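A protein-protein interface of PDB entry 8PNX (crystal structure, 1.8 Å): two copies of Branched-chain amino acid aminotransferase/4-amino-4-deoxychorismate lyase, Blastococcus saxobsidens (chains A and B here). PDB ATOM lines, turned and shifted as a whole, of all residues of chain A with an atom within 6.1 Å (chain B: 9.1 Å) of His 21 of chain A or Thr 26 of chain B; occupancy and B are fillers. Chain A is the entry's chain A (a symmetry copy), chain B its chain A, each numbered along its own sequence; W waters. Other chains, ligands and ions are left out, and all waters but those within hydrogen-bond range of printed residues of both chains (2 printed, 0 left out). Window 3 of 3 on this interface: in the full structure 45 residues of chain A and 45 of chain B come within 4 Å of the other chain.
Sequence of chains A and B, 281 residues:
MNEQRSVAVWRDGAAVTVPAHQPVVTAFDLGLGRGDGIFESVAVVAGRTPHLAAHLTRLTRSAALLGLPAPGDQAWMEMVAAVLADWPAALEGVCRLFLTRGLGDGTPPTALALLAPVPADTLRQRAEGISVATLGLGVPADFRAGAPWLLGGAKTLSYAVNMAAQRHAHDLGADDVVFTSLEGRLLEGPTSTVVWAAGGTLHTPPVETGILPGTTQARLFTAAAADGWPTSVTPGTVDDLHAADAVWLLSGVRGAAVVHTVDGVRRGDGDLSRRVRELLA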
ATOM      1  N   ARG A   5     -21.964  12.625 -15.033  1.00  0.00           N
ATOM      2  CA  ARG A   5     -20.700  13.399 -14.844  1.00  0.00           C
ATOM      3  C   ARG A   5     -20.799  14.696 -15.652  1.00  0.00           C
ATOM      4  O   ARG A   5     -21.512  14.715 -16.669  1.00  0.00           O
ATOM      5  CB  ARG A   5     -19.471  12.555 -15.225  1.00  0.00           C
ATOM      6  CG  ARG A   5     -19.116  11.468 -14.214  1.00  0.00           C
ATOM      7  CD  ARG A   5     -17.893  10.646 -14.608  1.00  0.00           C
ATOM      8  NE  ARG A   5     -17.846  10.445 -16.051  1.00  0.00           N
ATOM      9  CZ  ARG A   5     -16.788  10.032 -16.743  1.00  0.00           C
ATOM     10  NH1 ARG A   5     -15.648   9.751 -16.134  1.00  0.00           N
ATOM     11  NH2 ARG A   5     -16.878   9.916 -18.052  1.00  0.00           N
ATOM     12  N   VAL A   7     -18.471  18.448 -16.726  1.00  0.00           N
ATOM     13  CA  VAL A   7     -17.172  19.157 -16.695  1.00  0.00           C
ATOM     14  C   VAL A   7     -17.392  20.529 -17.326  1.00  0.00           C
ATOM     15  O   VAL A   7     -18.206  20.623 -18.277  1.00  0.00           O
ATOM     16  CB  VAL A   7     -16.081  18.359 -17.443  1.00  0.00           C
ATOM     17  CG1 VAL A   7     -14.775  19.106 -17.452  1.00  0.00           C
ATOM     18  CG2 VAL A   7     -15.906  16.944 -16.899  1.00  0.00           C
ATOM     19  N   VAL A  18     -18.176  20.994 -21.338  1.00  0.00           N
ATOM     20  CA  VAL A  18     -17.706  19.968 -22.322  1.00  0.00           C
ATOM     21  C   VAL A  18     -18.246  18.616 -21.878  1.00  0.00           C
ATOM     22  O   VAL A  18     -18.439  18.382 -20.692  1.00  0.00           O
ATOM     23  CB  VAL A  18     -16.174  19.903 -22.489  1.00  0.00           C
ATOM     24  CG1 VAL A  18     -15.563  21.250 -22.860  1.00  0.00           C
ATOM     25  CG2 VAL A  18     -15.480  19.318 -21.271  1.00  0.00           C
ATOM     26  N   PRO A  19     -18.456  17.639 -22.777  1.00  0.00           N
ATOM     27  CA  PRO A  19     -18.859  16.317 -22.322  1.00  0.00           C
ATOM     28  C   PRO A  19     -17.798  15.688 -21.391  1.00  0.00           C
ATOM     29  O   PRO A  19     -16.598  15.932 -21.553  1.00  0.00           O
ATOM     30  CB  PRO A  19     -19.110  15.546 -23.627  1.00  0.00           C
ATOM     31  CG  PRO A  19     -19.209  16.610 -24.707  1.00  0.00           C
ATOM     32  CD  PRO A  19     -18.294  17.722 -24.235  1.00  0.00           C
ATOM     33  N   ALA A  20     -18.264  14.888 -20.421  1.00  0.00           N
ATOM     34  CA  ALA A  20     -17.482  14.355 -19.280  1.00  0.00           C
ATOM     35  C   ALA A  20     -16.375  13.396 -19.756  1.00  0.00           C
ATOM     36  O   ALA A  20     -15.300  13.378 -19.130  1.00  0.00           O
ATOM     37  CB  ALA A  20     -18.414  13.710 -18.286  1.00  0.00           C
ATOM     38  N   HIS A  21     -16.606  12.655 -20.848  1.00  0.00           N
ATOM     39  CA  HIS A  21     -15.654  11.654 -21.410  1.00  0.00           C
ATOM     40  C   HIS A  21     -14.601  12.354 -22.281  1.00  0.00           C
ATOM     41  O   HIS A  21     -13.676  11.671 -22.726  1.00  0.00           O
ATOM     42  CB  HIS A  21     -16.419  10.572 -22.199  1.00  0.00           C
ATOM     43  CG  HIS A  21     -17.112  11.101 -23.417  1.00  0.00           C
ATOM     44  ND1 HIS A  21     -18.473  11.329 -23.453  1.00  0.00           N
ATOM     45  CD2 HIS A  21     -16.622  11.518 -24.613  1.00  0.00           C
ATOM     46  CE1 HIS A  21     -18.796  11.820 -24.641  1.00  0.00           C
ATOM     47  NE2 HIS A  21     -17.671  11.971 -25.362  1.00  0.00           N
ATOM     48  N   GLN A  22     -14.784  13.639 -22.596  1.00  0.00           N
ATOM     49  CA  GLN A  22     -13.918  14.394 -23.536  1.00  0.00           C
ATOM     50  C   GLN A  22     -12.639  14.835 -22.833  1.00  0.00           C
ATOM     51  O   GLN A  22     -12.682  15.485 -21.777  1.00  0.00           O
ATOM     52  CB  GLN A  22     -14.634  15.625 -24.083  1.00  0.00           C
ATOM     53  CG  GLN A  22     -13.875  16.334 -25.203  1.00  0.00           C
ATOM     54  CD  GLN A  22     -14.738  17.404 -25.812  1.00  0.00           C
ATOM     55  OE1 GLN A  22     -15.766  17.105 -26.426  1.00  0.00           O
ATOM     56  NE2 GLN A  22     -14.360  18.657 -25.596  1.00  0.00           N
ATOM     57  N   PRO A  23     -11.461  14.553 -23.442  1.00  0.00           N
ATOM     58  CA  PRO A  23     -10.184  15.007 -22.890  1.00  0.00           C
ATOM     59  C   PRO A  23     -10.189  16.526 -22.733  1.00  0.00           C
ATOM     60  O   PRO A  23     -10.695  17.206 -23.622  1.00  0.00           O
ATOM     61  CB  PRO A  23      -9.133  14.578 -23.939  1.00  0.00           C
ATOM     62  CG  PRO A  23      -9.800  13.461 -24.715  1.00  0.00           C
ATOM     63  CD  PRO A  23     -11.287  13.739 -24.659  1.00  0.00           C
ATOM     64  N   VAL A  24      -9.612  17.033 -21.642  1.00  0.00           N
ATOM     65  CA  VAL A  24      -9.565  18.492 -21.371  1.00  0.00           C
ATOM     66  C   VAL A  24      -8.142  18.945 -21.087  1.00  0.00           C
ATOM     67  O   VAL A  24      -7.881  20.132 -21.161  1.00  0.00           O
ATOM     68  CB  VAL A  24     -10.516  18.860 -20.215  1.00  0.00           C
ATOM     69  CG1 VAL A  24     -11.942  18.678 -20.654  1.00  0.00           C
ATOM     70  CG2 VAL A  24     -10.233  18.034 -18.970  1.00  0.00           C
ATOM     71  N   VAL A  25      -7.226  18.036 -20.813  1.00  0.00           N
ATOM     72  CA  VAL A  25      -5.857  18.462 -20.445  1.00  0.00           C
ATOM     73  C   VAL A  25      -4.901  17.828 -21.455  1.00  0.00           C
ATOM     74  O   VAL A  25      -5.116  16.659 -21.813  1.00  0.00           O
ATOM     75  CB  VAL A  25      -5.603  18.090 -18.972  1.00  0.00           C
ATOM     76  CG1 VAL A  25      -4.213  17.601 -18.710  1.00  0.00           C
ATOM     77  CG2 VAL A  25      -6.006  19.221 -18.021  1.00  0.00           C
ATOM     78  N   ARG B  11      -4.085   3.416 -27.319  1.00  0.00           N
ATOM     79  CA  ARG B  11      -5.499   3.388 -27.744  1.00  0.00           C
ATOM     80  C   ARG B  11      -5.781   2.051 -28.426  1.00  0.00           C
ATOM     81  O   ARG B  11      -5.251   1.856 -29.534  1.00  0.00           O
ATOM     82  CB  ARG B  11      -5.703   4.527 -28.743  1.00  0.00           C
ATOM     83  CG  ARG B  11      -7.123   4.671 -29.268  1.00  0.00           C
ATOM     84  CD  ARG B  11      -7.386   6.119 -29.657  1.00  0.00           C
ATOM     85  NE  ARG B  11      -7.273   6.970 -28.472  1.00  0.00           N
ATOM     86  CZ  ARG B  11      -7.268   8.299 -28.475  1.00  0.00           C
ATOM     87  NH1 ARG B  11      -7.357   8.967 -29.616  1.00  0.00           N
ATOM     88  NH2 ARG B  11      -7.167   8.954 -27.331  1.00  0.00           N
ATOM     89  N   PRO B  23      -6.002  18.067 -26.265  1.00  0.00           N
ATOM     90  CA  PRO B  23      -6.210  17.447 -24.956  1.00  0.00           C
ATOM     91  C   PRO B  23      -6.190  15.926 -25.085  1.00  0.00           C
ATOM     92  O   PRO B  23      -6.749  15.410 -26.050  1.00  0.00           O
ATOM     93  CB  PRO B  23      -7.610  17.930 -24.514  1.00  0.00           C
ATOM     94  CG  PRO B  23      -7.853  19.188 -25.322  1.00  0.00           C
ATOM     95  CD  PRO B  23      -7.074  19.020 -26.609  1.00  0.00           C
ATOM     96  N   VAL B  24      -5.583  15.235 -24.117  1.00  0.00           N
ATOM     97  CA  VAL B  24      -5.486  13.754 -24.138  1.00  0.00           C
ATOM     98  C   VAL B  24      -5.997  13.158 -22.835  1.00  0.00           C
ATOM     99  O   VAL B  24      -6.284  11.975 -22.806  1.00  0.00           O
ATOM    100  CB  VAL B  24      -4.040  13.309 -24.432  1.00  0.00           C
ATOM    101  CG1 VAL B  24      -3.681  13.656 -25.849  1.00  0.00           C
ATOM    102  CG2 VAL B  24      -3.050  13.937 -23.463  1.00  0.00           C
ATOM    103  N   VAL B  25      -6.157  13.950 -21.793  1.00  0.00           N
ATOM    104  CA  VAL B  25      -6.566  13.375 -20.491  1.00  0.00           C
ATOM    105  C   VAL B  25      -7.869  14.063 -20.085  1.00  0.00           C
ATOM    106  O   VAL B  25      -7.979  15.283 -20.291  1.00  0.00           O
ATOM    107  CB  VAL B  25      -5.401  13.527 -19.495  1.00  0.00           C
ATOM    108  CG1 VAL B  25      -5.843  13.869 -18.106  1.00  0.00           C
ATOM    109  CG2 VAL B  25      -4.467  12.314 -19.521  1.00  0.00           C
ATOM    110  N   THR B  26      -8.838  13.283 -19.615  1.00  0.00           N
ATOM    111  CA  THR B  26     -10.139  13.795 -19.109  1.00  0.00           C
ATOM    112  C   THR B  26      -9.965  14.341 -17.680  1.00  0.00           C
ATOM    113  O   THR B  26      -8.944  14.061 -16.997  1.00  0.00           O
ATOM    114  CB  THR B  26     -11.241  12.718 -19.132  1.00  0.00           C
ATOM    115  OG1 THR B  26     -11.074  11.907 -17.964  1.00  0.00           O
ATOM    116  CG2 THR B  26     -11.230  11.873 -20.402  1.00  0.00           C
ATOM    117  N   ALA B  27     -10.945  15.126 -17.231  1.00  0.00           N
ATOM    118  CA  ALA B  27     -10.963  15.764 -15.908  1.00  0.00           C
ATOM    119  C   ALA B  27     -10.836  14.700 -14.798  1.00  0.00           C
ATOM    120  O   ALA B  27     -10.338  15.032 -13.711  1.00  0.00           O
ATOM    121  CB  ALA B  27     -12.249  16.578 -15.814  1.00  0.00           C
ATOM    122  N   PHE B  28     -11.308  13.469 -15.036  1.00  0.00           N
ATOM    123  CA  PHE B  28     -11.464  12.436 -13.981  1.00  0.00           C
ATOM    124  C   PHE B  28     -10.236  11.532 -13.900  1.00  0.00           C
ATOM    125  O   PHE B  28     -10.196  10.680 -12.984  1.00  0.00           O
ATOM    126  CB  PHE B  28     -12.750  11.622 -14.208  1.00  0.00           C
ATOM    127  CG  PHE B  28     -13.973  12.473 -13.993  1.00  0.00           C
ATOM    128  CD1 PHE B  28     -14.401  12.746 -12.706  1.00  0.00           C
ATOM    129  CD2 PHE B  28     -14.581  13.131 -15.041  1.00  0.00           C
ATOM    130  CE1 PHE B  28     -15.489  13.589 -12.485  1.00  0.00           C
ATOM    131  CE2 PHE B  28     -15.687  13.956 -14.826  1.00  0.00           C
ATOM    132  CZ  PHE B  28     -16.135  14.187 -13.541  1.00  0.00           C
ATOM    133  N   ASP B  29      -9.256  11.726 -14.791  1.00  0.00           N
ATOM    134  CA  ASP B  29      -8.003  10.927 -14.777  1.00  0.00           C
ATOM    135  C   ASP B  29      -7.313  11.166 -13.422  1.00  0.00           C
ATOM    136  O   ASP B  29      -7.126  12.321 -13.015  1.00  0.00           O
ATOM    137  CB  ASP B  29      -7.121  11.275 -15.979  1.00  0.00           C
ATOM    138  CG  ASP B  29      -6.127  10.174 -16.247  1.00  0.00           C
ATOM    139  OD1 ASP B  29      -5.195   9.996 -15.405  1.00  0.00           O
ATOM    140  OD2 ASP B  29      -6.344   9.470 -17.238  1.00  0.00           O
ATOM    141  N   LEU B  30      -6.969  10.095 -12.715  1.00  0.00           N
ATOM    142  CA  LEU B  30      -6.354  10.150 -11.373  1.00  0.00           C
ATOM    143  C   LEU B  30      -4.905  10.623 -11.474  1.00  0.00           C
ATOM    144  O   LEU B  30      -4.411  11.107 -10.503  1.00  0.00           O
ATOM    145  CB  LEU B  30      -6.444   8.762 -10.750  1.00  0.00           C
ATOM    146  CG  LEU B  30      -7.843   8.395 -10.249  1.00  0.00           C
ATOM    147  CD1 LEU B  30      -7.883   6.918  -9.906  1.00  0.00           C
ATOM    148  CD2 LEU B  30      -8.231   9.262  -9.066  1.00  0.00           C
ATOM    149  N   GLY B  31      -4.283  10.573 -12.654  1.00  0.00           N
ATOM    150  CA  GLY B  31      -2.939  11.148 -12.843  1.00  0.00           C
ATOM    151  C   GLY B  31      -3.026  12.650 -12.683  1.00  0.00           C
ATOM    152  O   GLY B  31      -2.144  13.241 -12.075  1.00  0.00           O
ATOM    153  N   LEU B  32      -4.101  13.253 -13.178  1.00  0.00           N
ATOM    154  CA  LEU B  32      -4.321  14.699 -12.993  1.00  0.00           C
ATOM    155  C   LEU B  32      -4.826  15.010 -11.575  1.00  0.00           C
ATOM    156  O   LEU B  32      -4.234  15.907 -10.920  1.00  0.00           O
ATOM    157  CB  LEU B  32      -5.315  15.167 -14.039  1.00  0.00           C
ATOM    158  CG  LEU B  32      -5.861  16.571 -13.836  1.00  0.00           C
ATOM    159  CD1 LEU B  32      -4.741  17.544 -13.949  1.00  0.00           C
ATOM    160  CD2 LEU B  32      -6.963  16.851 -14.863  1.00  0.00           C
ATOM    161  N   GLY B  33      -5.905  14.366 -11.123  1.00  0.00           N
ATOM    162  CA  GLY B  33      -6.597  14.818  -9.891  1.00  0.00           C
ATOM    163  C   GLY B  33      -5.901  14.399  -8.620  1.00  0.00           C
ATOM    164  O   GLY B  33      -6.102  15.086  -7.560  1.00  0.00           O
ATOM    165  N   THR B 100      -0.817   6.471 -15.739  1.00  0.00           N
ATOM    166  CA  THR B 100      -1.687   6.926 -14.626  1.00  0.00           C
ATOM    167  C   THR B 100      -2.634   5.794 -14.227  1.00  0.00           C
ATOM    168  O   THR B 100      -2.871   4.852 -15.056  1.00  0.00           O
ATOM    169  CB  THR B 100      -2.461   8.209 -14.975  1.00  0.00           C
ATOM    170  OG1 THR B 100      -3.676   7.802 -15.615  1.00  0.00           O
ATOM    171  CG2 THR B 100      -1.696   9.181 -15.866  1.00  0.00           C
ATOM    172  N   GLY B 102      -5.622   6.146 -14.293  1.00  0.00           N
ATOM    173  CA  GLY B 102      -6.803   6.354 -15.150  1.00  0.00           C
ATOM    174  C   GLY B 102      -8.001   6.749 -14.321  1.00  0.00           C
ATOM    175  O   GLY B 102      -7.847   7.582 -13.445  1.00  0.00           O
ATOM    176  N   LEU B 103      -9.161   6.177 -14.629  1.00  0.00           N
ATOM    177  CA  LEU B 103     -10.451   6.517 -13.976  1.00  0.00           C
ATOM    178  C   LEU B 103     -10.572   5.769 -12.643  1.00  0.00           C
ATOM    179  O   LEU B 103     -11.450   6.135 -11.861  1.00  0.00           O
ATOM    180  CB  LEU B 103     -11.584   6.169 -14.944  1.00  0.00           C
ATOM    181  CG  LEU B 103     -11.634   7.007 -16.224  1.00  0.00           C
ATOM    182  CD1 LEU B 103     -12.932   6.754 -16.997  1.00  0.00           C
ATOM    183  CD2 LEU B 103     -11.459   8.490 -15.922  1.00  0.00           C
ATOM    184  N   THR B 110      -4.013   4.868 -17.977  1.00  0.00           N
ATOM    185  CA  THR B 110      -3.739   5.755 -19.133  1.00  0.00           C
ATOM    186  C   THR B 110      -2.246   5.721 -19.464  1.00  0.00           C
ATOM    187  O   THR B 110      -1.442   5.991 -18.569  1.00  0.00           O
ATOM    188  CB  THR B 110      -4.122   7.190 -18.794  1.00  0.00           C
ATOM    189  OG1 THR B 110      -5.501   7.142 -18.419  1.00  0.00           O
ATOM    190  CG2 THR B 110      -3.858   8.163 -19.927  1.00  0.00           C
HETATM  191  O   HOH W   1     -13.616  11.147 -17.963  1.00  0.00           O
HETATM  192  O   HOH W   2     -13.315  15.396 -19.120  1.00  0.00           O
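Printed residues of chain B within 4 Å of Arg 5 of chain A: Phe 28 (3.7 Å). Ala 20 of chain A touches none of the printed residues of chain B. Printed residues of chain B within 4 Å of Val 24 of chain A: Pro 23 (3.6 Å), Val 25 (2.7 Å), Thr 26 (3.9 Å) and Ala 27 (3.5 Å). Of chain A, only His 21 (3.4 Å), Pro 23 (3.9 Å) and Val 24 (3.9 Å) come within 4 Å of Thr 26 of chain B. Gly 31 of chain B touches none of the printed residues of chain A. The nearest residue of chain B that does not touch His 21 of chain A is Phe 28 of chain B (6.2 Å). The nearest residue of chain A that does not touch Thr 26 of chain B is Gln 22 of chain A (4.1 Å).
Of the 10 printed residues of chain A, 6 touch a printed residue of chain B. Printed residues of chain A that touch a printed residue of chain B: Arg 5, Val 7, His 21, Pro 23, Val 24 and Val 25. Of the 16 printed residues of chain B, 6 touch a printed residue of chain A. Hydrophobic or aromatic side chains of chain B that line the printed part of chain A: Pro 23, Val 24, Val 25, Ala 27 and Phe 28. Among the printed residues, 15 pairs touch across the chains. Among the printed residues, no Asp or Glu carboxylate lies within 4 Å of a Lys or Arg side-chain nitrogen of the other chain.
The backbone NH (N) of Phe 28 of chain B lies close to the side-chain hydroxyl (OG1) of Thr 26 of chain B (3.3 Å). O of Val 7 of chain A is in hydrogen-bond range of N of Val 18 of chain A, at 3.1 Å.
N of Val 24 of chain A is in hydrogen-bond range of O of Val 25 of chain B (2.7 Å). The backbone NH (N) of Val 24 of chain B lies within hydrogen-bond range of the backbone carbonyl oxygen (O) of Val 25 of chain A, 2.7 Å away. O of Val 25 of chain A sits at hydrogen-bond distance from N of Val 25 of chain B, at 2.9 Å.
Arg 5 of chain A touches Phe 28 of chain B (NH1 to CD2, 3.7 Å). Val 7 of chain A touches Phe 28 of chain B (CG2 to CE2, 3.6 Å). His 21 of chain A touches Thr 26 of chain B (O to CG2, 3.4 Å). Pro 23 of chain B touches Pro 23 of chain A (O to CB, 3.3 Å). Pro 23 of chain A touches Val 24 of chain B. Pro 23 of chain A touches Val 25 of chain B. Thr 26 of chain B touches Pro 23 of chain A. Val 24 of chain A touches Pro 23 of chain B (C to CB, 3.6 Å). Thr 26 of chain B touches Val 24 of chain A (C to CG2, 3.9 Å). Val 24 of chain A touches Ala 27 of chain B (CG2 to N, 3.5 Å).
Water W1 lies within hydrogen-bond range of the side-chain hydroxyl of Thr 26 of chain B, the backbone carbonyl oxygen of Ala 20 of chain A and the guanidinium group of Arg 5 of chain A. Water W2 lies within hydrogen-bond range of O of Gln 22 of chain A (2.7 Å), O of Ala 20 of chain A (2.8 Å) and N of Ala 27 of chain B (3.0 Å).
Pro 23 of chain B touches its own counterpart, Pro 23 of chain A. Pro 23 of chain A touches Val 25 of chain B, and with the chains exchanged Val 25 of chain A touches Pro 23 of chain B. Val 24 of chain A touches Val 25 of chain B, and with the chains exchanged Val 25 of chain A touches Val 24 of chain B. Val 25 of chain A touches its own counterpart, Val 25 of chain B. Positions printed for both chains: 23, 24 and 25. Of the 15 pairs that touch across the chains among the printed residues, 8 have their exchanged pair printed and touching as well.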
